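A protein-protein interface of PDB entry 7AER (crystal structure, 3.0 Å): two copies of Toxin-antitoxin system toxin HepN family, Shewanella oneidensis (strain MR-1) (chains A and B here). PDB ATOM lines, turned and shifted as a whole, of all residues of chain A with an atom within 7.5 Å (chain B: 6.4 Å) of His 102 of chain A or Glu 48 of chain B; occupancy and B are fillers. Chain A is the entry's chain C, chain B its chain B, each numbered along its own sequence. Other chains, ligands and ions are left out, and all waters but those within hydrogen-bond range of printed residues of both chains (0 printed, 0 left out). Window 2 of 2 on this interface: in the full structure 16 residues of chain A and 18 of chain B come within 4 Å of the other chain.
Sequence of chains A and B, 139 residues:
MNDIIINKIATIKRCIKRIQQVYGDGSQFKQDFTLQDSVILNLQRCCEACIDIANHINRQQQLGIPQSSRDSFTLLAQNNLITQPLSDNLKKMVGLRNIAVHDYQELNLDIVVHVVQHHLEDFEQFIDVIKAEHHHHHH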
ATOM      1  N   GLN A  44     -16.326 -32.622  -3.337  1.00  0.00           N
ATOM      2  CA  GLN A  44     -16.148 -31.225  -2.958  1.00  0.00           C
ATOM      3  C   GLN A  44     -15.993 -30.343  -4.191  1.00  0.00           C
ATOM      4  O   GLN A  44     -16.556 -29.243  -4.248  1.00  0.00           O
ATOM      5  CB  GLN A  44     -14.942 -31.097  -2.031  1.00  0.00           C
ATOM      6  CG  GLN A  44     -14.420 -29.690  -1.863  1.00  0.00           C
ATOM      7  CD  GLN A  44     -13.164 -29.649  -1.024  1.00  0.00           C
ATOM      8  OE1 GLN A  44     -12.404 -28.681  -1.067  1.00  0.00           O
ATOM      9  NE2 GLN A  44     -12.935 -30.707  -0.253  1.00  0.00           N
ATOM     10  N   GLU A  48     -18.075 -26.991  -5.077  1.00  0.00           N
ATOM     11  CA  GLU A  48     -17.413 -25.719  -5.346  1.00  0.00           C
ATOM     12  C   GLU A  48     -17.749 -25.203  -6.740  1.00  0.00           C
ATOM     13  O   GLU A  48     -17.865 -23.989  -6.942  1.00  0.00           O
ATOM     14  CB  GLU A  48     -15.899 -25.895  -5.219  1.00  0.00           C
ATOM     15  CG  GLU A  48     -15.389 -26.320  -3.841  1.00  0.00           C
ATOM     16  CD  GLU A  48     -15.527 -25.248  -2.784  1.00  0.00           C
ATOM     17  OE1 GLU A  48     -15.634 -24.058  -3.148  1.00  0.00           O
ATOM     18  OE2 GLU A  48     -15.503 -25.593  -1.583  1.00  0.00           O
ATOM     19  N   SER A  69     -22.994 -20.111   2.007  1.00  0.00           N
ATOM     20  CA  SER A  69     -22.873 -20.856   0.758  1.00  0.00           C
ATOM     21  C   SER A  69     -24.201 -21.488   0.364  1.00  0.00           C
ATOM     22  O   SER A  69     -24.522 -21.583  -0.826  1.00  0.00           O
ATOM     23  CB  SER A  69     -21.785 -21.923   0.879  1.00  0.00           C
ATOM     24  OG  SER A  69     -20.492 -21.344   0.875  1.00  0.00           O
ATOM     25  N   GLY A  95     -23.685 -28.709   2.952  1.00  0.00           N
ATOM     26  CA  GLY A  95     -23.408 -29.188   4.296  1.00  0.00           C
ATOM     27  C   GLY A  95     -22.360 -30.284   4.316  1.00  0.00           C
ATOM     28  O   GLY A  95     -21.468 -30.287   5.166  1.00  0.00           O
ATOM     29  N   LEU A  96     -22.451 -31.230   3.377  1.00  0.00           N
ATOM     30  CA  LEU A  96     -21.433 -32.271   3.273  1.00  0.00           C
ATOM     31  C   LEU A  96     -20.076 -31.676   2.919  1.00  0.00           C
ATOM     32  O   LEU A  96     -19.045 -32.094   3.461  1.00  0.00           O
ATOM     33  CB  LEU A  96     -21.848 -33.312   2.231  1.00  0.00           C
ATOM     34  CG  LEU A  96     -20.819 -34.397   1.898  1.00  0.00           C
ATOM     35  CD1 LEU A  96     -20.504 -35.239   3.124  1.00  0.00           C
ATOM     36  CD2 LEU A  96     -21.290 -35.274   0.746  1.00  0.00           C
ATOM     37  N   ARG A  97     -20.059 -30.700   2.008  1.00  0.00           N
ATOM     38  CA  ARG A  97     -18.810 -30.038   1.643  1.00  0.00           C
ATOM     39  C   ARG A  97     -18.193 -29.323   2.838  1.00  0.00           C
ATOM     40  O   ARG A  97     -16.969 -29.337   3.015  1.00  0.00           O
ATOM     41  CB  ARG A  97     -19.062 -29.058   0.497  1.00  0.00           C
ATOM     42  CG  ARG A  97     -18.078 -27.901   0.427  1.00  0.00           C
ATOM     43  CD  ARG A  97     -18.511 -26.882  -0.612  1.00  0.00           C
ATOM     44  NE  ARG A  97     -17.659 -25.701  -0.612  1.00  0.00           N
ATOM     45  CZ  ARG A  97     -17.961 -24.559  -0.002  1.00  0.00           C
ATOM     46  NH1 ARG A  97     -19.104 -24.442   0.660  1.00  0.00           N
ATOM     47  NH2 ARG A  97     -17.122 -23.535  -0.057  1.00  0.00           N
ATOM     48  N   ASN A  98     -19.025 -28.699   3.675  1.00  0.00           N
ATOM     49  CA  ASN A  98     -18.500 -27.934   4.802  1.00  0.00           C
ATOM     50  C   ASN A  98     -17.890 -28.844   5.863  1.00  0.00           C
ATOM     51  O   ASN A  98     -16.893 -28.480   6.496  1.00  0.00           O
ATOM     52  CB  ASN A  98     -19.604 -27.066   5.408  1.00  0.00           C
ATOM     53  CG  ASN A  98     -19.955 -25.877   4.534  1.00  0.00           C
ATOM     54  OD1 ASN A  98     -19.169 -25.468   3.682  1.00  0.00           O
ATOM     55  ND2 ASN A  98     -21.136 -25.311   4.751  1.00  0.00           N
ATOM     56  N   ILE A  99     -18.472 -30.028   6.075  1.00  0.00           N
ATOM     57  CA  ILE A  99     -17.908 -30.953   7.053  1.00  0.00           C
ATOM     58  C   ILE A  99     -16.558 -31.478   6.579  1.00  0.00           C
ATOM     59  O   ILE A  99     -15.649 -31.698   7.390  1.00  0.00           O
ATOM     60  CB  ILE A  99     -18.891 -32.104   7.340  1.00  0.00           C
ATOM     61  CG1 ILE A  99     -20.250 -31.559   7.782  1.00  0.00           C
ATOM     62  CG2 ILE A  99     -18.341 -33.023   8.417  1.00  0.00           C
ATOM     63  CD1 ILE A  99     -20.237 -30.924   9.150  1.00  0.00           C
ATOM     64  N   ALA A 100     -16.393 -31.678   5.270  1.00  0.00           N
ATOM     65  CA  ALA A 100     -15.126 -32.191   4.759  1.00  0.00           C
ATOM     66  C   ALA A 100     -14.041 -31.122   4.788  1.00  0.00           C
ATOM     67  O   ALA A 100     -12.894 -31.403   5.157  1.00  0.00           O
ATOM     68  CB  ALA A 100     -15.310 -32.732   3.343  1.00  0.00           C
ATOM     69  N   VAL A 101     -14.382 -29.892   4.402  1.00  0.00           N
ATOM     70  CA  VAL A 101     -13.399 -28.811   4.391  1.00  0.00           C
ATOM     71  C   VAL A 101     -13.098 -28.353   5.814  1.00  0.00           C
ATOM     72  O   VAL A 101     -11.959 -28.440   6.287  1.00  0.00           O
ATOM     73  CB  VAL A 101     -13.890 -27.645   3.517  1.00  0.00           C
ATOM     74  CG1 VAL A 101     -12.939 -26.462   3.625  1.00  0.00           C
ATOM     75  CG2 VAL A 101     -14.028 -28.094   2.070  1.00  0.00           C
ATOM     76  N   HIS A 102     -14.115 -27.856   6.512  1.00  0.00           N
ATOM     77  CA  HIS A 102     -13.962 -27.410   7.890  1.00  0.00           C
ATOM     78  C   HIS A 102     -14.286 -28.558   8.834  1.00  0.00           C
ATOM     79  O   HIS A 102     -15.312 -29.227   8.681  1.00  0.00           O
ATOM     80  CB  HIS A 102     -14.865 -26.213   8.176  1.00  0.00           C
ATOM     81  CG  HIS A 102     -14.698 -25.091   7.201  1.00  0.00           C
ATOM     82  ND1 HIS A 102     -15.633 -24.805   6.229  1.00  0.00           N
ATOM     83  CD2 HIS A 102     -13.697 -24.194   7.036  1.00  0.00           C
ATOM     84  CE1 HIS A 102     -15.218 -23.775   5.513  1.00  0.00           C
ATOM     85  NE2 HIS A 102     -14.046 -23.386   5.983  1.00  0.00           N
ATOM     86  N   ASP A 103     -13.412 -28.779   9.810  1.00  0.00           N
ATOM     87  CA  ASP A 103     -13.513 -29.945  10.685  1.00  0.00           C
ATOM     88  C   ASP A 103     -14.296 -29.583  11.948  1.00  0.00           C
ATOM     89  O   ASP A 103     -13.756 -29.471  13.050  1.00  0.00           O
ATOM     90  CB  ASP A 103     -12.121 -30.471  11.014  1.00  0.00           C
ATOM     91  CG  ASP A 103     -12.147 -31.876  11.571  1.00  0.00           C
ATOM     92  OD1 ASP A 103     -13.232 -32.493  11.572  1.00  0.00           O
ATOM     93  OD2 ASP A 103     -11.081 -32.362  12.007  1.00  0.00           O
ATOM     94  N   TYR A 104     -15.608 -29.400  11.769  1.00  0.00           N
ATOM     95  CA  TYR A 104     -16.502 -29.142  12.893  1.00  0.00           C
ATOM     96  C   TYR A 104     -17.472 -30.293  13.136  1.00  0.00           C
ATOM     97  O   TYR A 104     -18.490 -30.111  13.811  1.00  0.00           O
ATOM     98  CB  TYR A 104     -17.250 -27.819  12.704  1.00  0.00           C
ATOM     99  CG  TYR A 104     -18.265 -27.743  11.577  1.00  0.00           C
ATOM    100  CD1 TYR A 104     -17.867 -27.523  10.264  1.00  0.00           C
ATOM    101  CD2 TYR A 104     -19.627 -27.829  11.839  1.00  0.00           C
ATOM    102  CE1 TYR A 104     -18.797 -27.427   9.238  1.00  0.00           C
ATOM    103  CE2 TYR A 104     -20.563 -27.734  10.821  1.00  0.00           C
ATOM    104  CZ  TYR A 104     -20.144 -27.532   9.521  1.00  0.00           C
ATOM    105  OH  TYR A 104     -21.073 -27.435   8.504  1.00  0.00           O
ATOM    106  N   GLN A 105     -17.157 -31.477  12.614  1.00  0.00           N
ATOM    107  CA  GLN A 105     -17.892 -32.712  12.857  1.00  0.00           C
ATOM    108  C   GLN A 105     -17.084 -33.868  12.290  1.00  0.00           C
ATOM    109  O   GLN A 105     -16.364 -33.707  11.300  1.00  0.00           O
ATOM    110  CB  GLN A 105     -19.289 -32.687  12.224  1.00  0.00           C
ATOM    111  CG  GLN A 105     -20.426 -32.557  13.224  1.00  0.00           C
ATOM    112  CD  GLN A 105     -21.789 -32.781  12.595  1.00  0.00           C
ATOM    113  OE1 GLN A 105     -22.111 -33.886  12.157  1.00  0.00           O
ATOM    114  NE2 GLN A 105     -22.598 -31.728  12.547  1.00  0.00           N
ATOM    115  N   GLU A 106     -17.205 -35.029  12.930  1.00  0.00           N
ATOM    116  CA  GLU A 106     -16.592 -36.242  12.402  1.00  0.00           C
ATOM    117  C   GLU A 106     -17.328 -36.666  11.138  1.00  0.00           C
ATOM    118  O   GLU A 106     -18.548 -36.865  11.160  1.00  0.00           O
ATOM    119  CB  GLU A 106     -16.625 -37.354  13.447  1.00  0.00           C
ATOM    120  N   LEU A 107     -16.593 -36.795  10.036  1.00  0.00           N
ATOM    121  CA  LEU A 107     -17.213 -37.087   8.749  1.00  0.00           C
ATOM    122  C   LEU A 107     -17.854 -38.470   8.760  1.00  0.00           C
ATOM    123  O   LEU A 107     -17.202 -39.471   9.073  1.00  0.00           O
ATOM    124  CB  LEU A 107     -16.172 -36.990   7.632  1.00  0.00           C
ATOM    125  CG  LEU A 107     -16.697 -36.893   6.198  1.00  0.00           C
ATOM    126  CD1 LEU A 107     -17.568 -35.660   6.030  1.00  0.00           C
ATOM    127  CD2 LEU A 107     -15.545 -36.870   5.209  1.00  0.00           C
ATOM    128  N   LYS B   8      -5.904 -30.079  16.246  1.00  0.00           N
ATOM    129  CA  LYS B   8      -5.474 -29.709  14.903  1.00  0.00           C
ATOM    130  C   LYS B   8      -4.046 -30.169  14.633  1.00  0.00           C
ATOM    131  O   LYS B   8      -3.731 -30.605  13.521  1.00  0.00           O
ATOM    132  CB  LYS B   8      -5.606 -28.200  14.704  1.00  0.00           C
ATOM    133  CG  LYS B   8      -7.042 -27.713  14.733  1.00  0.00           C
ATOM    134  CD  LYS B   8      -7.851 -28.330  13.607  1.00  0.00           C
ATOM    135  CE  LYS B   8      -9.261 -27.767  13.568  1.00  0.00           C
ATOM    136  NZ  LYS B   8     -10.030 -28.289  12.407  1.00  0.00           N
ATOM    137  N   LEU B  43      -3.408 -32.565   1.813  1.00  0.00           N
ATOM    138  CA  LEU B  43      -2.747 -31.265   1.797  1.00  0.00           C
ATOM    139  C   LEU B  43      -3.714 -30.160   2.200  1.00  0.00           C
ATOM    140  O   LEU B  43      -3.332 -29.210   2.896  1.00  0.00           O
ATOM    141  CB  LEU B  43      -2.166 -30.985   0.410  1.00  0.00           C
ATOM    142  CG  LEU B  43      -0.759 -31.501   0.107  1.00  0.00           C
ATOM    143  CD1 LEU B  43      -0.400 -31.219  -1.341  1.00  0.00           C
ATOM    144  CD2 LEU B  43       0.255 -30.864   1.048  1.00  0.00           C
ATOM    145  N   GLN B  44      -4.973 -30.269   1.768  1.00  0.00           N
ATOM    146  CA  GLN B  44      -5.995 -29.310   2.175  1.00  0.00           C
ATOM    147  C   GLN B  44      -6.306 -29.439   3.660  1.00  0.00           C
ATOM    148  O   GLN B  44      -6.454 -28.431   4.361  1.00  0.00           O
ATOM    149  CB  GLN B  44      -7.259 -29.517   1.342  1.00  0.00           C
ATOM    150  CG  GLN B  44      -8.513 -28.873   1.916  1.00  0.00           C
ATOM    151  CD  GLN B  44      -9.755 -29.221   1.114  1.00  0.00           C
ATOM    152  OE1 GLN B  44     -10.880 -29.110   1.606  1.00  0.00           O
ATOM    153  NE2 GLN B  44      -9.556 -29.650  -0.127  1.00  0.00           N
ATOM    154  N   ARG B  45      -6.419 -30.676   4.151  1.00  0.00           N
ATOM    155  CA  ARG B  45      -6.675 -30.890   5.570  1.00  0.00           C
ATOM    156  C   ARG B  45      -5.562 -30.298   6.423  1.00  0.00           C
ATOM    157  O   ARG B  45      -5.817 -29.816   7.533  1.00  0.00           O
ATOM    158  CB  ARG B  45      -6.833 -32.385   5.840  1.00  0.00           C
ATOM    159  CG  ARG B  45      -8.120 -32.981   5.288  1.00  0.00           C
ATOM    160  CD  ARG B  45      -8.075 -34.502   5.296  1.00  0.00           C
ATOM    161  NE  ARG B  45      -9.387 -35.090   5.044  1.00  0.00           N
ATOM    162  CZ  ARG B  45      -9.590 -36.372   4.763  1.00  0.00           C
ATOM    163  NH1 ARG B  45      -8.563 -37.208   4.691  1.00  0.00           N
ATOM    164  NH2 ARG B  45     -10.820 -36.819   4.549  1.00  0.00           N
ATOM    165  N   CYS B  46      -4.323 -30.335   5.927  1.00  0.00           N
ATOM    166  CA  CYS B  46      -3.224 -29.677   6.623  1.00  0.00           C
ATOM    167  C   CYS B  46      -3.375 -28.160   6.576  1.00  0.00           C
ATOM    168  O   CYS B  46      -3.172 -27.478   7.588  1.00  0.00           O
ATOM    169  CB  CYS B  46      -1.885 -30.097   6.012  1.00  0.00           C
ATOM    170  SG  CYS B  46      -1.368 -31.789   6.394  1.00  0.00           S
ATOM    171  N   CYS B  47      -3.722 -27.618   5.406  1.00  0.00           N
ATOM    172  CA  CYS B  47      -3.858 -26.171   5.258  1.00  0.00           C
ATOM    173  C   CYS B  47      -4.955 -25.618   6.158  1.00  0.00           C
ATOM    174  O   CYS B  47      -4.740 -24.649   6.896  1.00  0.00           O
ATOM    175  CB  CYS B  47      -4.151 -25.822   3.799  1.00  0.00           C
ATOM    176  SG  CYS B  47      -2.734 -25.929   2.693  1.00  0.00           S
ATOM    177  N   GLU B  48      -6.146 -26.221   6.104  1.00  0.00           N
ATOM    178  CA  GLU B  48      -7.266 -25.730   6.899  1.00  0.00           C
ATOM    179  C   GLU B  48      -6.987 -25.824   8.390  1.00  0.00           C
ATOM    180  O   GLU B  48      -7.456 -24.980   9.161  1.00  0.00           O
ATOM    181  CB  GLU B  48      -8.538 -26.500   6.547  1.00  0.00           C
ATOM    182  CG  GLU B  48      -8.993 -26.291   5.114  1.00  0.00           C
ATOM    183  CD  GLU B  48      -9.488 -24.880   4.859  1.00  0.00           C
ATOM    184  OE1 GLU B  48      -9.459 -24.446   3.690  1.00  0.00           O
ATOM    185  OE2 GLU B  48      -9.887 -24.199   5.828  1.00  0.00           O
ATOM    186  N   ALA B  49      -6.227 -26.832   8.817  1.00  0.00           N
ATOM    187  CA  ALA B  49      -5.917 -26.952  10.238  1.00  0.00           C
ATOM    188  C   ALA B  49      -4.939 -25.870  10.673  1.00  0.00           C
ATOM    189  O   ALA B  49      -5.040 -25.349  11.790  1.00  0.00           O
ATOM    190  CB  ALA B  49      -5.366 -28.343  10.542  1.00  0.00           C
ATOM    191  N   CYS B  50      -3.993 -25.510   9.801  1.00  0.00           N
ATOM    192  CA  CYS B  50      -3.104 -24.394  10.105  1.00  0.00           C
ATOM    193  C   CYS B  50      -3.868 -23.078  10.103  1.00  0.00           C
ATOM    194  O   CYS B  50      -3.605 -22.198  10.931  1.00  0.00           O
ATOM    195  CB  CYS B  50      -1.953 -24.341   9.100  1.00  0.00           C
ATOM    196  SG  CYS B  50      -0.792 -25.717   9.205  1.00  0.00           S
ATOM    197  N   ILE B  51      -4.810 -22.922   9.171  1.00  0.00           N
ATOM    198  CA  ILE B  51      -5.644 -21.725   9.151  1.00  0.00           C
ATOM    199  C   ILE B  51      -6.500 -21.664  10.410  1.00  0.00           C
ATOM    200  O   ILE B  51      -6.709 -20.591  10.989  1.00  0.00           O
ATOM    201  CB  ILE B  51      -6.501 -21.693   7.870  1.00  0.00           C
ATOM    202  CG1 ILE B  51      -5.608 -21.544   6.634  1.00  0.00           C
ATOM    203  CG2 ILE B  51      -7.508 -20.561   7.920  1.00  0.00           C
ATOM    204  CD1 ILE B  51      -6.358 -21.641   5.318  1.00  0.00           C
ATOM    205  N   ASP B  52      -6.998 -22.819  10.863  1.00  0.00           N
ATOM    206  CA  ASP B  52      -7.789 -22.857  12.091  1.00  0.00           C
ATOM    207  C   ASP B  52      -6.939 -22.519  13.310  1.00  0.00           C
ATOM    208  O   ASP B  52      -7.380 -21.772  14.191  1.00  0.00           O
ATOM    209  CB  ASP B  52      -8.441 -24.230  12.252  1.00  0.00           C
ATOM    210  CG  ASP B  52      -9.500 -24.493  11.201  1.00  0.00           C
ATOM    211  OD1 ASP B  52     -10.040 -23.514  10.645  1.00  0.00           O
ATOM    212  OD2 ASP B  52      -9.786 -25.677  10.925  1.00  0.00           O
ATOM    213  N   ILE B  53      -5.724 -23.069  13.383  1.00  0.00           N
ATOM    214  CA  ILE B  53      -4.819 -22.729  14.477  1.00  0.00           C
ATOM    215  C   ILE B  53      -4.475 -21.248  14.435  1.00  0.00           C
ATOM    216  O   ILE B  53      -4.430 -20.572  15.471  1.00  0.00           O
ATOM    217  CB  ILE B  53      -3.551 -23.601  14.418  1.00  0.00           C
ATOM    218  CG1 ILE B  53      -3.888 -25.068  14.685  1.00  0.00           C
ATOM    219  CG2 ILE B  53      -2.510 -23.105  15.411  1.00  0.00           C
ATOM    220  CD1 ILE B  53      -2.699 -25.994  14.548  1.00  0.00           C
ATOM    221  N   ASN B  55      -6.252 -18.751  13.196  1.00  0.00           N
ATOM    222  CA  ASN B  55      -7.381 -17.900  13.559  1.00  0.00           C
ATOM    223  C   ASN B  55      -7.674 -17.951  15.051  1.00  0.00           C
ATOM    224  O   ASN B  55      -8.160 -16.966  15.618  1.00  0.00           O
ATOM    225  CB  ASN B  55      -8.626 -18.308  12.773  1.00  0.00           C
ATOM    226  CG  ASN B  55      -8.541 -17.926  11.315  1.00  0.00           C
ATOM    227  OD1 ASN B  55      -8.323 -16.763  10.978  1.00  0.00           O
ATOM    228  ND2 ASN B  55      -8.726 -18.902  10.437  1.00  0.00           N
ATOM    229  N   SER B  69      -7.925 -15.822   4.585  1.00  0.00           N
ATOM    230  CA  SER B  69      -7.125 -16.888   5.175  1.00  0.00           C
ATOM    231  C   SER B  69      -5.662 -16.483   5.270  1.00  0.00           C
ATOM    232  O   SER B  69      -4.989 -16.785   6.263  1.00  0.00           O
ATOM    233  CB  SER B  69      -7.264 -18.167   4.349  1.00  0.00           C
ATOM    234  OG  SER B  69      -8.622 -18.544   4.203  1.00  0.00           O
ATOM    235  N   ARG B  97      -3.857 -24.908  -2.518  1.00  0.00           N
ATOM    236  CA  ARG B  97      -5.117 -25.539  -2.141  1.00  0.00           C
ATOM    237  C   ARG B  97      -6.265 -25.050  -3.016  1.00  0.00           C
ATOM    238  O   ARG B  97      -7.082 -25.852  -3.483  1.00  0.00           O
ATOM    239  CB  ARG B  97      -5.418 -25.270  -0.666  1.00  0.00           C
ATOM    240  CG  ARG B  97      -6.830 -25.649  -0.246  1.00  0.00           C
ATOM    241  CD  ARG B  97      -7.614 -24.426   0.205  1.00  0.00           C
ATOM    242  NE  ARG B  97      -8.952 -24.388  -0.379  1.00  0.00           N
ATOM    243  CZ  ARG B  97     -10.064 -24.724   0.267  1.00  0.00           C
ATOM    244  NH1 ARG B  97     -10.008 -25.120   1.532  1.00  0.00           N
ATOM    245  NH2 ARG B  97     -11.235 -24.658  -0.350  1.00  0.00           N
ATOM    246  N   ASN B  98      -6.340 -23.739  -3.255  1.00  0.00           N
ATOM    247  CA  ASN B  98      -7.457 -23.194  -4.020  1.00  0.00           C
ATOM    248  C   ASN B  98      -7.377 -23.591  -5.489  1.00  0.00           C
ATOM    249  O   ASN B  98      -8.397 -23.917  -6.105  1.00  0.00           O
ATOM    250  CB  ASN B  98      -7.498 -21.674  -3.880  1.00  0.00           C
ATOM    251  CG  ASN B  98      -7.803 -21.225  -2.465  1.00  0.00           C
ATOM    252  OD1 ASN B  98      -8.426 -21.953  -1.692  1.00  0.00           O
ATOM    253  ND2 ASN B  98      -7.371 -20.019  -2.121  1.00  0.00           N
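Among the printed residues, pairs that only touch across the chains: Asp 103 of chain A with Lys 8 of chain B, Val 101 of chain A with Gln 44 of chain B, Val 101 of chain A with Arg 97 of chain B, Val 101 of chain A with Glu 48 of chain B and His 102 of chain A with Glu 48 of chain B.
Of the printed residues of chain B, Gln 44 of chain A touches Gln 44 (3.1 Å). Printed residues of chain B within 4 Å of Val 101 of chain A: Gln 44, Glu 48 and Arg 97. Of the printed residues of chain B, His 102 of chain A touches Glu 48 (3.997 Å). Of the printed residues of chain B, Asp 103 of chain A touches Lys 8 (3.3 Å). Leu 107 of chain A touches none of the printed residues of chain B. Of the printed residues of chain A, Arg 97 of chain B touches Val 101. The nearest printed residue of chain A that does not touch Glu 48 of chain B is Asp 103 of chain A (6.3 Å). The nearest printed residue of chain B that does not touch Asp 103 of chain A is Asp 52 of chain B (4.9 Å).
Of the 16 printed residues of chain A, 4 touch a printed residue of chain B. Of the 16 printed residues of chain B, 4 touch a printed residue of chain A. Printed residues of chain B that touch a printed residue of chain A: Lys 8, Gln 44, Glu 48 and Arg 97. Among the printed residues, no Asp or Glu carboxylate lies within 4 Å of a Lys or Arg side-chain nitrogen of the other chain.
Gln 44 of chain A touches its own counterpart, Gln 44 of chain B. Positions printed for both chains: 44, 48, 69, 97 and 98. Of the 6 pairs that touch across the chains among the printed residues, 1 has its exchanged pair printed and touching as well.
The guanidinium group (NE) of Arg 97 of chain B is in hydrogen-bond range of the side-chain amide oxygen (OD1) of Asn 98 of chain B (2.8 Å). The side-chain amino group (NZ) of Lys 8 of chain B is in salt-bridge range of the side-chain carboxylate (OD2) of Asp 52 of chain B (3.0 Å).
OE1 of Gln 44 of chain B lies close to OE1 of Gln 44 of chain A, 3.1 Å away.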
